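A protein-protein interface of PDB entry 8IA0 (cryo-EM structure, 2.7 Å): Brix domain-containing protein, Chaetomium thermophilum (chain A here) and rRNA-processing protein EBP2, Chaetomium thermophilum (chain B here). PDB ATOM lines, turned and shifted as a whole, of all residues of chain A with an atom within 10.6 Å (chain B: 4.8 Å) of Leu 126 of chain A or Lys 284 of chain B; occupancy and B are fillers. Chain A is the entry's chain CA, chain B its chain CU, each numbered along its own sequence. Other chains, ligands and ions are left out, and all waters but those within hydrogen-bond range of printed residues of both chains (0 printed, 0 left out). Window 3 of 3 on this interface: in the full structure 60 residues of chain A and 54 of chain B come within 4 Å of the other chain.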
ATOM      1  N   ARG A  47     -14.232  -1.440  23.146  1.00  0.00           N
ATOM      2  CA  ARG A  47     -12.904  -2.042  23.184  1.00  0.00           C
ATOM      3  C   ARG A  47     -12.052  -1.427  24.285  1.00  0.00           C
ATOM      4  O   ARG A  47     -11.305  -2.137  24.968  1.00  0.00           O
ATOM      5  CB  ARG A  47     -12.220  -1.889  21.828  1.00  0.00           C
ATOM      6  CG  ARG A  47     -11.000  -2.777  21.647  1.00  0.00           C
ATOM      7  CD  ARG A  47     -10.404  -2.620  20.260  1.00  0.00           C
ATOM      8  NE  ARG A  47     -11.273  -3.170  19.228  1.00  0.00           N
ATOM      9  CZ  ARG A  47     -11.332  -4.455  18.903  1.00  0.00           C
ATOM     10  NH1 ARG A  47     -10.579  -5.356  19.514  1.00  0.00           N
ATOM     11  NH2 ARG A  47     -12.167  -4.845  17.944  1.00  0.00           N
ATOM     12  N   HIS A 121      -5.718  -5.426  21.956  1.00  0.00           N
ATOM     13  CA  HIS A 121      -6.254  -6.776  21.785  1.00  0.00           C
ATOM     14  C   HIS A 121      -6.611  -7.287  23.176  1.00  0.00           C
ATOM     15  O   HIS A 121      -5.769  -7.870  23.864  1.00  0.00           O
ATOM     16  CB  HIS A 121      -5.259  -7.696  21.090  1.00  0.00           C
ATOM     17  CG  HIS A 121      -5.209  -7.519  19.607  1.00  0.00           C
ATOM     18  ND1 HIS A 121      -6.047  -8.199  18.748  1.00  0.00           N
ATOM     19  CD2 HIS A 121      -4.426  -6.738  18.827  1.00  0.00           C
ATOM     20  CE1 HIS A 121      -5.779  -7.844  17.505  1.00  0.00           C
ATOM     21  NE2 HIS A 121      -4.799  -6.959  17.525  1.00  0.00           N
ATOM     22  N   THR A 122      -7.856  -7.067  23.582  1.00  0.00           N
ATOM     23  CA  THR A 122      -8.292  -7.387  24.930  1.00  0.00           C
ATOM     24  C   THR A 122      -8.450  -8.895  25.096  1.00  0.00           C
ATOM     25  O   THR A 122      -8.142  -9.685  24.201  1.00  0.00           O
ATOM     26  CB  THR A 122      -9.601  -6.668  25.246  1.00  0.00           C
ATOM     27  OG1 THR A 122     -10.651  -7.213  24.439  1.00  0.00           O
ATOM     28  CG2 THR A 122      -9.473  -5.183  24.956  1.00  0.00           C
ATOM     29  N   MET A 123      -8.938  -9.302  26.263  1.00  0.00           N
ATOM     30  CA  MET A 123      -9.305 -10.691  26.474  1.00  0.00           C
ATOM     31  C   MET A 123     -10.542 -11.024  25.641  1.00  0.00           C
ATOM     32  O   MET A 123     -11.030 -10.215  24.845  1.00  0.00           O
ATOM     33  CB  MET A 123      -9.568 -10.965  27.952  1.00  0.00           C
ATOM     34  CG  MET A 123      -8.400 -11.555  28.725  1.00  0.00           C
ATOM     35  SD  MET A 123      -8.347 -10.931  30.417  1.00  0.00           S
ATOM     36  CE  MET A 123      -6.598 -10.993  30.771  1.00  0.00           C
ATOM     37  N   GLU A 124     -11.052 -12.240  25.823  1.00  0.00           N
ATOM     38  CA  GLU A 124     -12.252 -12.722  25.143  1.00  0.00           C
ATOM     39  C   GLU A 124     -12.085 -12.770  23.628  1.00  0.00           C
ATOM     40  O   GLU A 124     -13.063 -12.963  22.899  1.00  0.00           O
ATOM     41  CB  GLU A 124     -13.489 -11.894  25.514  1.00  0.00           C
ATOM     42  CG  GLU A 124     -13.539 -11.441  26.966  1.00  0.00           C
ATOM     43  CD  GLU A 124     -14.949 -11.140  27.434  1.00  0.00           C
ATOM     44  OE1 GLU A 124     -15.875 -11.887  27.055  1.00  0.00           O
ATOM     45  OE2 GLU A 124     -15.131 -10.156  28.182  1.00  0.00           O
ATOM     46  N   GLU A 125     -10.865 -12.590  23.135  1.00  0.00           N
ATOM     47  CA  GLU A 125     -10.526 -12.872  21.748  1.00  0.00           C
ATOM     48  C   GLU A 125     -10.023 -14.306  21.688  1.00  0.00           C
ATOM     49  O   GLU A 125      -9.046 -14.652  22.359  1.00  0.00           O
ATOM     50  CB  GLU A 125      -9.472 -11.898  21.224  1.00  0.00           C
ATOM     51  CG  GLU A 125      -9.744 -10.445  21.568  1.00  0.00           C
ATOM     52  CD  GLU A 125      -9.399  -9.503  20.432  1.00  0.00           C
ATOM     53  OE1 GLU A 125      -8.419  -9.775  19.709  1.00  0.00           O
ATOM     54  OE2 GLU A 125     -10.106  -8.486  20.266  1.00  0.00           O
ATOM     55  N   LEU A 126     -10.688 -15.139  20.891  1.00  0.00           N
ATOM     56  CA  LEU A 126     -10.483 -16.577  20.997  1.00  0.00           C
ATOM     57  C   LEU A 126      -9.243 -17.047  20.251  1.00  0.00           C
ATOM     58  O   LEU A 126      -9.306 -18.011  19.486  1.00  0.00           O
ATOM     59  CB  LEU A 126     -11.714 -17.323  20.478  1.00  0.00           C
ATOM     60  CG  LEU A 126     -13.072 -16.765  20.902  1.00  0.00           C
ATOM     61  CD1 LEU A 126     -14.195 -17.483  20.177  1.00  0.00           C
ATOM     62  CD2 LEU A 126     -13.246 -16.870  22.406  1.00  0.00           C
ATOM     63  N   HIS A 127      -8.101 -16.407  20.497  1.00  0.00           N
ATOM     64  CA  HIS A 127      -6.850 -16.867  19.906  1.00  0.00           C
ATOM     65  C   HIS A 127      -5.687 -16.746  20.881  1.00  0.00           C
ATOM     66  O   HIS A 127      -4.540 -16.583  20.447  1.00  0.00           O
ATOM     67  CB  HIS A 127      -6.531 -16.100  18.619  1.00  0.00           C
ATOM     68  CG  HIS A 127      -6.272 -14.641  18.829  1.00  0.00           C
ATOM     69  ND1 HIS A 127      -5.004 -14.127  18.987  1.00  0.00           N
ATOM     70  CD2 HIS A 127      -7.118 -13.588  18.902  1.00  0.00           C
ATOM     71  CE1 HIS A 127      -5.080 -12.818  19.151  1.00  0.00           C
ATOM     72  NE2 HIS A 127      -6.352 -12.466  19.103  1.00  0.00           N
ATOM     73  N   PHE A 128      -5.947 -16.825  22.184  1.00  0.00           N
ATOM     74  CA  PHE A 128      -4.909 -16.672  23.193  1.00  0.00           C
ATOM     75  C   PHE A 128      -4.501 -17.991  23.834  1.00  0.00           C
ATOM     76  O   PHE A 128      -3.304 -18.245  23.998  1.00  0.00           O
ATOM     77  CB  PHE A 128      -5.371 -15.689  24.271  1.00  0.00           C
ATOM     78  CG  PHE A 128      -5.249 -14.250  23.861  1.00  0.00           C
ATOM     79  CD1 PHE A 128      -4.082 -13.777  23.289  1.00  0.00           C
ATOM     80  CD2 PHE A 128      -6.303 -13.373  24.035  1.00  0.00           C
ATOM     81  CE1 PHE A 128      -3.966 -12.456  22.905  1.00  0.00           C
ATOM     82  CE2 PHE A 128      -6.190 -12.051  23.652  1.00  0.00           C
ATOM     83  CZ  PHE A 128      -5.020 -11.593  23.087  1.00  0.00           C
ATOM     84  N   GLN A 129      -5.465 -18.836  24.197  1.00  0.00           N
ATOM     85  CA  GLN A 129      -5.248 -20.192  24.698  1.00  0.00           C
ATOM     86  C   GLN A 129      -4.592 -20.235  26.070  1.00  0.00           C
ATOM     87  O   GLN A 129      -4.132 -21.302  26.491  1.00  0.00           O
ATOM     88  CB  GLN A 129      -4.412 -21.033  23.727  1.00  0.00           C
ATOM     89  CG  GLN A 129      -5.009 -21.172  22.343  1.00  0.00           C
ATOM     90  CD  GLN A 129      -3.979 -21.570  21.312  1.00  0.00           C
ATOM     91  OE1 GLN A 129      -3.145 -22.441  21.555  1.00  0.00           O
ATOM     92  NE2 GLN A 129      -4.029 -20.931  20.150  1.00  0.00           N
ATOM     93  N   GLY A 130      -4.533 -19.114  26.786  1.00  0.00           N
ATOM     94  CA  GLY A 130      -3.922 -19.088  28.092  1.00  0.00           C
ATOM     95  C   GLY A 130      -4.857 -18.490  29.126  1.00  0.00           C
ATOM     96  O   GLY A 130      -5.793 -17.758  28.806  1.00  0.00           O
ATOM     97  N   ASN A 131      -4.579 -18.819  30.385  1.00  0.00           N
ATOM     98  CA  ASN A 131      -5.380 -18.343  31.500  1.00  0.00           C
ATOM     99  C   ASN A 131      -4.512 -18.301  32.746  1.00  0.00           C
ATOM    100  O   ASN A 131      -3.460 -18.941  32.814  1.00  0.00           O
ATOM    101  CB  ASN A 131      -6.608 -19.229  31.725  1.00  0.00           C
ATOM    102  CG  ASN A 131      -7.833 -18.436  32.121  1.00  0.00           C
ATOM    103  OD1 ASN A 131      -7.751 -17.240  32.383  1.00  0.00           O
ATOM    104  ND2 ASN A 131      -8.979 -19.100  32.163  1.00  0.00           N
ATOM    105  N   ILE A 232       2.476 -19.081  27.306  1.00  0.00           N
ATOM    106  CA  ILE A 232       1.324 -18.919  26.427  1.00  0.00           C
ATOM    107  C   ILE A 232       0.709 -17.559  26.721  1.00  0.00           C
ATOM    108  O   ILE A 232       0.481 -17.221  27.887  1.00  0.00           O
ATOM    109  CB  ILE A 232       0.286 -20.037  26.622  1.00  0.00           C
ATOM    110  CG1 ILE A 232       0.940 -21.410  26.482  1.00  0.00           C
ATOM    111  CG2 ILE A 232      -0.850 -19.889  25.629  1.00  0.00           C
ATOM    112  CD1 ILE A 232       0.394 -22.442  27.437  1.00  0.00           C
ATOM    113  N   GLU A 233       0.451 -16.778  25.674  1.00  0.00           N
ATOM    114  CA  GLU A 233      -0.173 -15.471  25.851  1.00  0.00           C
ATOM    115  C   GLU A 233      -1.616 -15.637  26.307  1.00  0.00           C
ATOM    116  O   GLU A 233      -2.338 -16.504  25.809  1.00  0.00           O
ATOM    117  CB  GLU A 233      -0.114 -14.683  24.545  1.00  0.00           C
ATOM    118  CG  GLU A 233       0.206 -13.214  24.723  1.00  0.00           C
ATOM    119  CD  GLU A 233       0.067 -12.431  23.437  1.00  0.00           C
ATOM    120  OE1 GLU A 233      -0.162 -13.057  22.381  1.00  0.00           O
ATOM    121  OE2 GLU A 233       0.188 -11.190  23.480  1.00  0.00           O
ATOM    122  N   ILE A 234      -2.042 -14.810  27.263  1.00  0.00           N
ATOM    123  CA  ILE A 234      -3.356 -15.011  27.865  1.00  0.00           C
ATOM    124  C   ILE A 234      -4.218 -13.760  27.805  1.00  0.00           C
ATOM    125  O   ILE A 234      -5.451 -13.849  27.809  1.00  0.00           O
ATOM    126  CB  ILE A 234      -3.226 -15.480  29.325  1.00  0.00           C
ATOM    127  CG1 ILE A 234      -2.867 -14.325  30.248  1.00  0.00           C
ATOM    128  CG2 ILE A 234      -2.132 -16.475  29.451  1.00  0.00           C
ATOM    129  CD1 ILE A 234      -2.705 -14.754  31.678  1.00  0.00           C
ATOM    130  N   GLY A 235      -3.592 -12.590  27.751  1.00  0.00           N
ATOM    131  CA  GLY A 235      -4.296 -11.387  28.113  1.00  0.00           C
ATOM    132  C   GLY A 235      -4.165 -10.235  27.149  1.00  0.00           C
ATOM    133  O   GLY A 235      -3.939 -10.407  25.947  1.00  0.00           O
ATOM    134  N   ARG A 237      -3.101  -7.146  24.870  1.00  0.00           N
ATOM    135  CA  ARG A 237      -1.935  -6.896  24.028  1.00  0.00           C
ATOM    136  C   ARG A 237      -2.116  -5.493  23.458  1.00  0.00           C
ATOM    137  O   ARG A 237      -3.017  -5.262  22.648  1.00  0.00           O
ATOM    138  CB  ARG A 237      -1.819  -7.954  22.937  1.00  0.00           C
ATOM    139  CG  ARG A 237      -1.101  -7.520  21.678  1.00  0.00           C
ATOM    140  CD  ARG A 237      -1.174  -8.608  20.619  1.00  0.00           C
ATOM    141  NE  ARG A 237      -0.200  -9.667  20.853  1.00  0.00           N
ATOM    142  CZ  ARG A 237      -0.087 -10.757  20.105  1.00  0.00           C
ATOM    143  NH1 ARG A 237      -0.879 -10.969  19.068  1.00  0.00           N
ATOM    144  NH2 ARG A 237       0.844 -11.656  20.408  1.00  0.00           N
ATOM    145  N   ALA B 280     -16.851 -20.011  30.176  1.00  0.00           N
ATOM    146  CA  ALA B 280     -17.482 -19.912  28.865  1.00  0.00           C
ATOM    147  C   ALA B 280     -16.498 -19.421  27.813  1.00  0.00           C
ATOM    148  O   ALA B 280     -16.504 -19.903  26.675  1.00  0.00           O
ATOM    149  CB  ALA B 280     -18.698 -18.989  28.937  1.00  0.00           C
ATOM    150  N   THR B 281     -15.651 -18.454  28.172  1.00  0.00           N
ATOM    151  CA  THR B 281     -14.660 -17.948  27.229  1.00  0.00           C
ATOM    152  C   THR B 281     -13.683 -19.040  26.815  1.00  0.00           C
ATOM    153  O   THR B 281     -13.382 -19.196  25.626  1.00  0.00           O
ATOM    154  CB  THR B 281     -13.911 -16.765  27.842  1.00  0.00           C
ATOM    155  OG1 THR B 281     -14.763 -15.614  27.855  1.00  0.00           O
ATOM    156  CG2 THR B 281     -12.659 -16.448  27.043  1.00  0.00           C
ATOM    157  N   MET B 282     -13.188 -19.818  27.778  1.00  0.00           N
ATOM    158  CA  MET B 282     -12.217 -20.854  27.449  1.00  0.00           C
ATOM    159  C   MET B 282     -12.876 -22.060  26.794  1.00  0.00           C
ATOM    160  O   MET B 282     -12.201 -22.836  26.110  1.00  0.00           O
ATOM    161  CB  MET B 282     -11.446 -21.273  28.699  1.00  0.00           C
ATOM    162  CG  MET B 282     -10.552 -20.178  29.254  1.00  0.00           C
ATOM    163  SD  MET B 282      -9.160 -19.805  28.174  1.00  0.00           S
ATOM    164  CE  MET B 282      -7.947 -20.992  28.729  1.00  0.00           C
ATOM    165  N   GLU B 283     -14.182 -22.243  26.996  1.00  0.00           N
ATOM    166  CA  GLU B 283     -14.899 -23.265  26.242  1.00  0.00           C
ATOM    167  C   GLU B 283     -15.027 -22.866  24.780  1.00  0.00           C
ATOM    168  O   GLU B 283     -14.956 -23.716  23.886  1.00  0.00           O
ATOM    169  CB  GLU B 283     -16.276 -23.511  26.856  1.00  0.00           C
ATOM    170  CG  GLU B 283     -16.882 -24.850  26.483  1.00  0.00           C
ATOM    171  CD  GLU B 283     -16.686 -25.902  27.556  1.00  0.00           C
ATOM    172  OE1 GLU B 283     -16.713 -25.545  28.752  1.00  0.00           O
ATOM    173  OE2 GLU B 283     -16.504 -27.086  27.204  1.00  0.00           O
ATOM    174  N   LYS B 284     -15.222 -21.572  24.517  1.00  0.00           N
ATOM    175  CA  LYS B 284     -15.221 -21.085  23.142  1.00  0.00           C
ATOM    176  C   LYS B 284     -13.846 -21.244  22.508  1.00  0.00           C
ATOM    177  O   LYS B 284     -13.737 -21.561  21.318  1.00  0.00           O
ATOM    178  CB  LYS B 284     -15.662 -19.623  23.104  1.00  0.00           C
ATOM    179  CG  LYS B 284     -17.101 -19.388  23.522  1.00  0.00           C
ATOM    180  CD  LYS B 284     -17.473 -17.921  23.404  1.00  0.00           C
ATOM    181  CE  LYS B 284     -18.917 -17.752  22.976  1.00  0.00           C
ATOM    182  NZ  LYS B 284     -19.784 -18.838  23.508  1.00  0.00           N
ATOM    183  N   VAL B 285     -12.786 -21.018  23.284  1.00  0.00           N
ATOM    184  CA  VAL B 285     -11.429 -21.141  22.757  1.00  0.00           C
ATOM    185  C   VAL B 285     -11.134 -22.588  22.384  1.00  0.00           C
ATOM    186  O   VAL B 285     -10.551 -22.868  21.329  1.00  0.00           O
ATOM    187  CB  VAL B 285     -10.410 -20.597  23.773  1.00  0.00           C
ATOM    188  CG1 VAL B 285      -8.994 -20.943  23.349  1.00  0.00           C
ATOM    189  CG2 VAL B 285     -10.567 -19.096  23.922  1.00  0.00           C
ATOM    190  N   LYS B 286     -11.532 -23.529  23.241  1.00  0.00           N
ATOM    191  CA  LYS B 286     -11.315 -24.941  22.935  1.00  0.00           C
ATOM    192  C   LYS B 286     -12.120 -25.373  21.717  1.00  0.00           C
ATOM    193  O   LYS B 286     -11.634 -26.149  20.887  1.00  0.00           O
ATOM    194  CB  LYS B 286     -11.669 -25.808  24.142  1.00  0.00           C
ATOM    195  CG  LYS B 286     -10.844 -27.079  24.240  1.00  0.00           C
ATOM    196  CD  LYS B 286     -11.719 -28.311  24.394  1.00  0.00           C
ATOM    197  CE  LYS B 286     -12.821 -28.088  25.412  1.00  0.00           C
ATOM    198  NZ  LYS B 286     -13.453 -29.368  25.832  1.00  0.00           N
ATOM    199  N   GLN B 287     -13.356 -24.884  21.593  1.00  0.00           N
ATOM    200  CA  GLN B 287     -14.195 -25.276  20.466  1.00  0.00           C
ATOM    201  C   GLN B 287     -13.598 -24.823  19.141  1.00  0.00           C
ATOM    202  O   GLN B 287     -13.648 -25.560  18.149  1.00  0.00           O
ATOM    203  CB  GLN B 287     -15.606 -24.714  20.637  1.00  0.00           C
ATOM    204  CG  GLN B 287     -16.467 -25.491  21.614  1.00  0.00           C
ATOM    205  CD  GLN B 287     -16.519 -26.972  21.293  1.00  0.00           C
ATOM    206  OE1 GLN B 287     -16.732 -27.364  20.146  1.00  0.00           O
ATOM    207  NE2 GLN B 287     -16.324 -27.804  22.309  1.00  0.00           N
ATOM    208  N   LYS B 288     -13.037 -23.612  19.096  1.00  0.00           N
ATOM    209  CA  LYS B 288     -12.440 -23.138  17.853  1.00  0.00           C
ATOM    210  C   LYS B 288     -11.223 -23.974  17.477  1.00  0.00           C
ATOM    211  O   LYS B 288     -10.999 -24.262  16.296  1.00  0.00           O
ATOM    212  CB  LYS B 288     -12.072 -21.657  17.962  1.00  0.00           C
ATOM    213  CG  LYS B 288     -11.100 -21.205  16.890  1.00  0.00           C
ATOM    214  CD  LYS B 288     -11.421 -19.814  16.376  1.00  0.00           C
ATOM    215  CE  LYS B 288     -10.381 -18.805  16.809  1.00  0.00           C
ATOM    216  NZ  LYS B 288     -10.274 -17.663  15.863  1.00  0.00           N
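Thr 281 of chain B touches Glu 124 of chain A.
CD2 of Leu 126 of chain A touches O of Thr 281 of chain B, at 3.97 Å.
Leu 126 of chain A touches Lys 284 of chain B (CD2 to CB, 3.7 Å).
CG2 of Val 285 of chain B touches CD2 of Leu 126 of chain A, at 3.8 Å.
O of Leu 126 of chain A touches CE of Lys 288 of chain B, at 3.0 Å.
O of Gly 130 of chain A touches CE of Met 282 of chain B, at 3.9 Å.
CG of Met 282 of chain B touches ND2 of Asn 131 of chain A, 3.5 Å away.
Of the printed residues of chain B, Glu 124 of chain A touches Thr 281.
Leu 126 of chain A touches four residues of chain B.
Gln 129 of chain A touches none of the printed residues of chain B.
Printed residues of chain B within 4 Å of Asn 131 of chain A: Met 282.
Ile 234 of chain A touches none of the printed residues of chain B.
Of the printed residues of chain A, Thr 281 of chain B touches Glu 124 and Leu 126.
Printed residues of chain A within 4 Å of Met 282 of chain B: Gly 130 and Asn 131.
No residue of chain A comes within 4 Å of Glu 283 of chain B.
Of the printed residues of chain A, Lys 288 of chain B touches Leu 126 (3.0 Å).
The nearest printed residue of chain B that does not touch Leu 126 of chain A is Met 282 of chain B (6.1 Å).
The nearest residue of chain A that does not touch Lys 284 of chain B is Glu 124 of chain A (6.7 Å).
Of the 17 printed residues of chain A, 4 touch a printed residue of chain B.
Of the 9 printed residues of chain B, 5 touch a printed residue of chain A.
Hydrophobic or aromatic side chains of chain B that line the printed part of chain A: Met 282 and Val 285.
Among the printed residues, no Asp or Glu carboxylate lies within 4 Å of a Lys or Arg side-chain nitrogen of the other chain.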
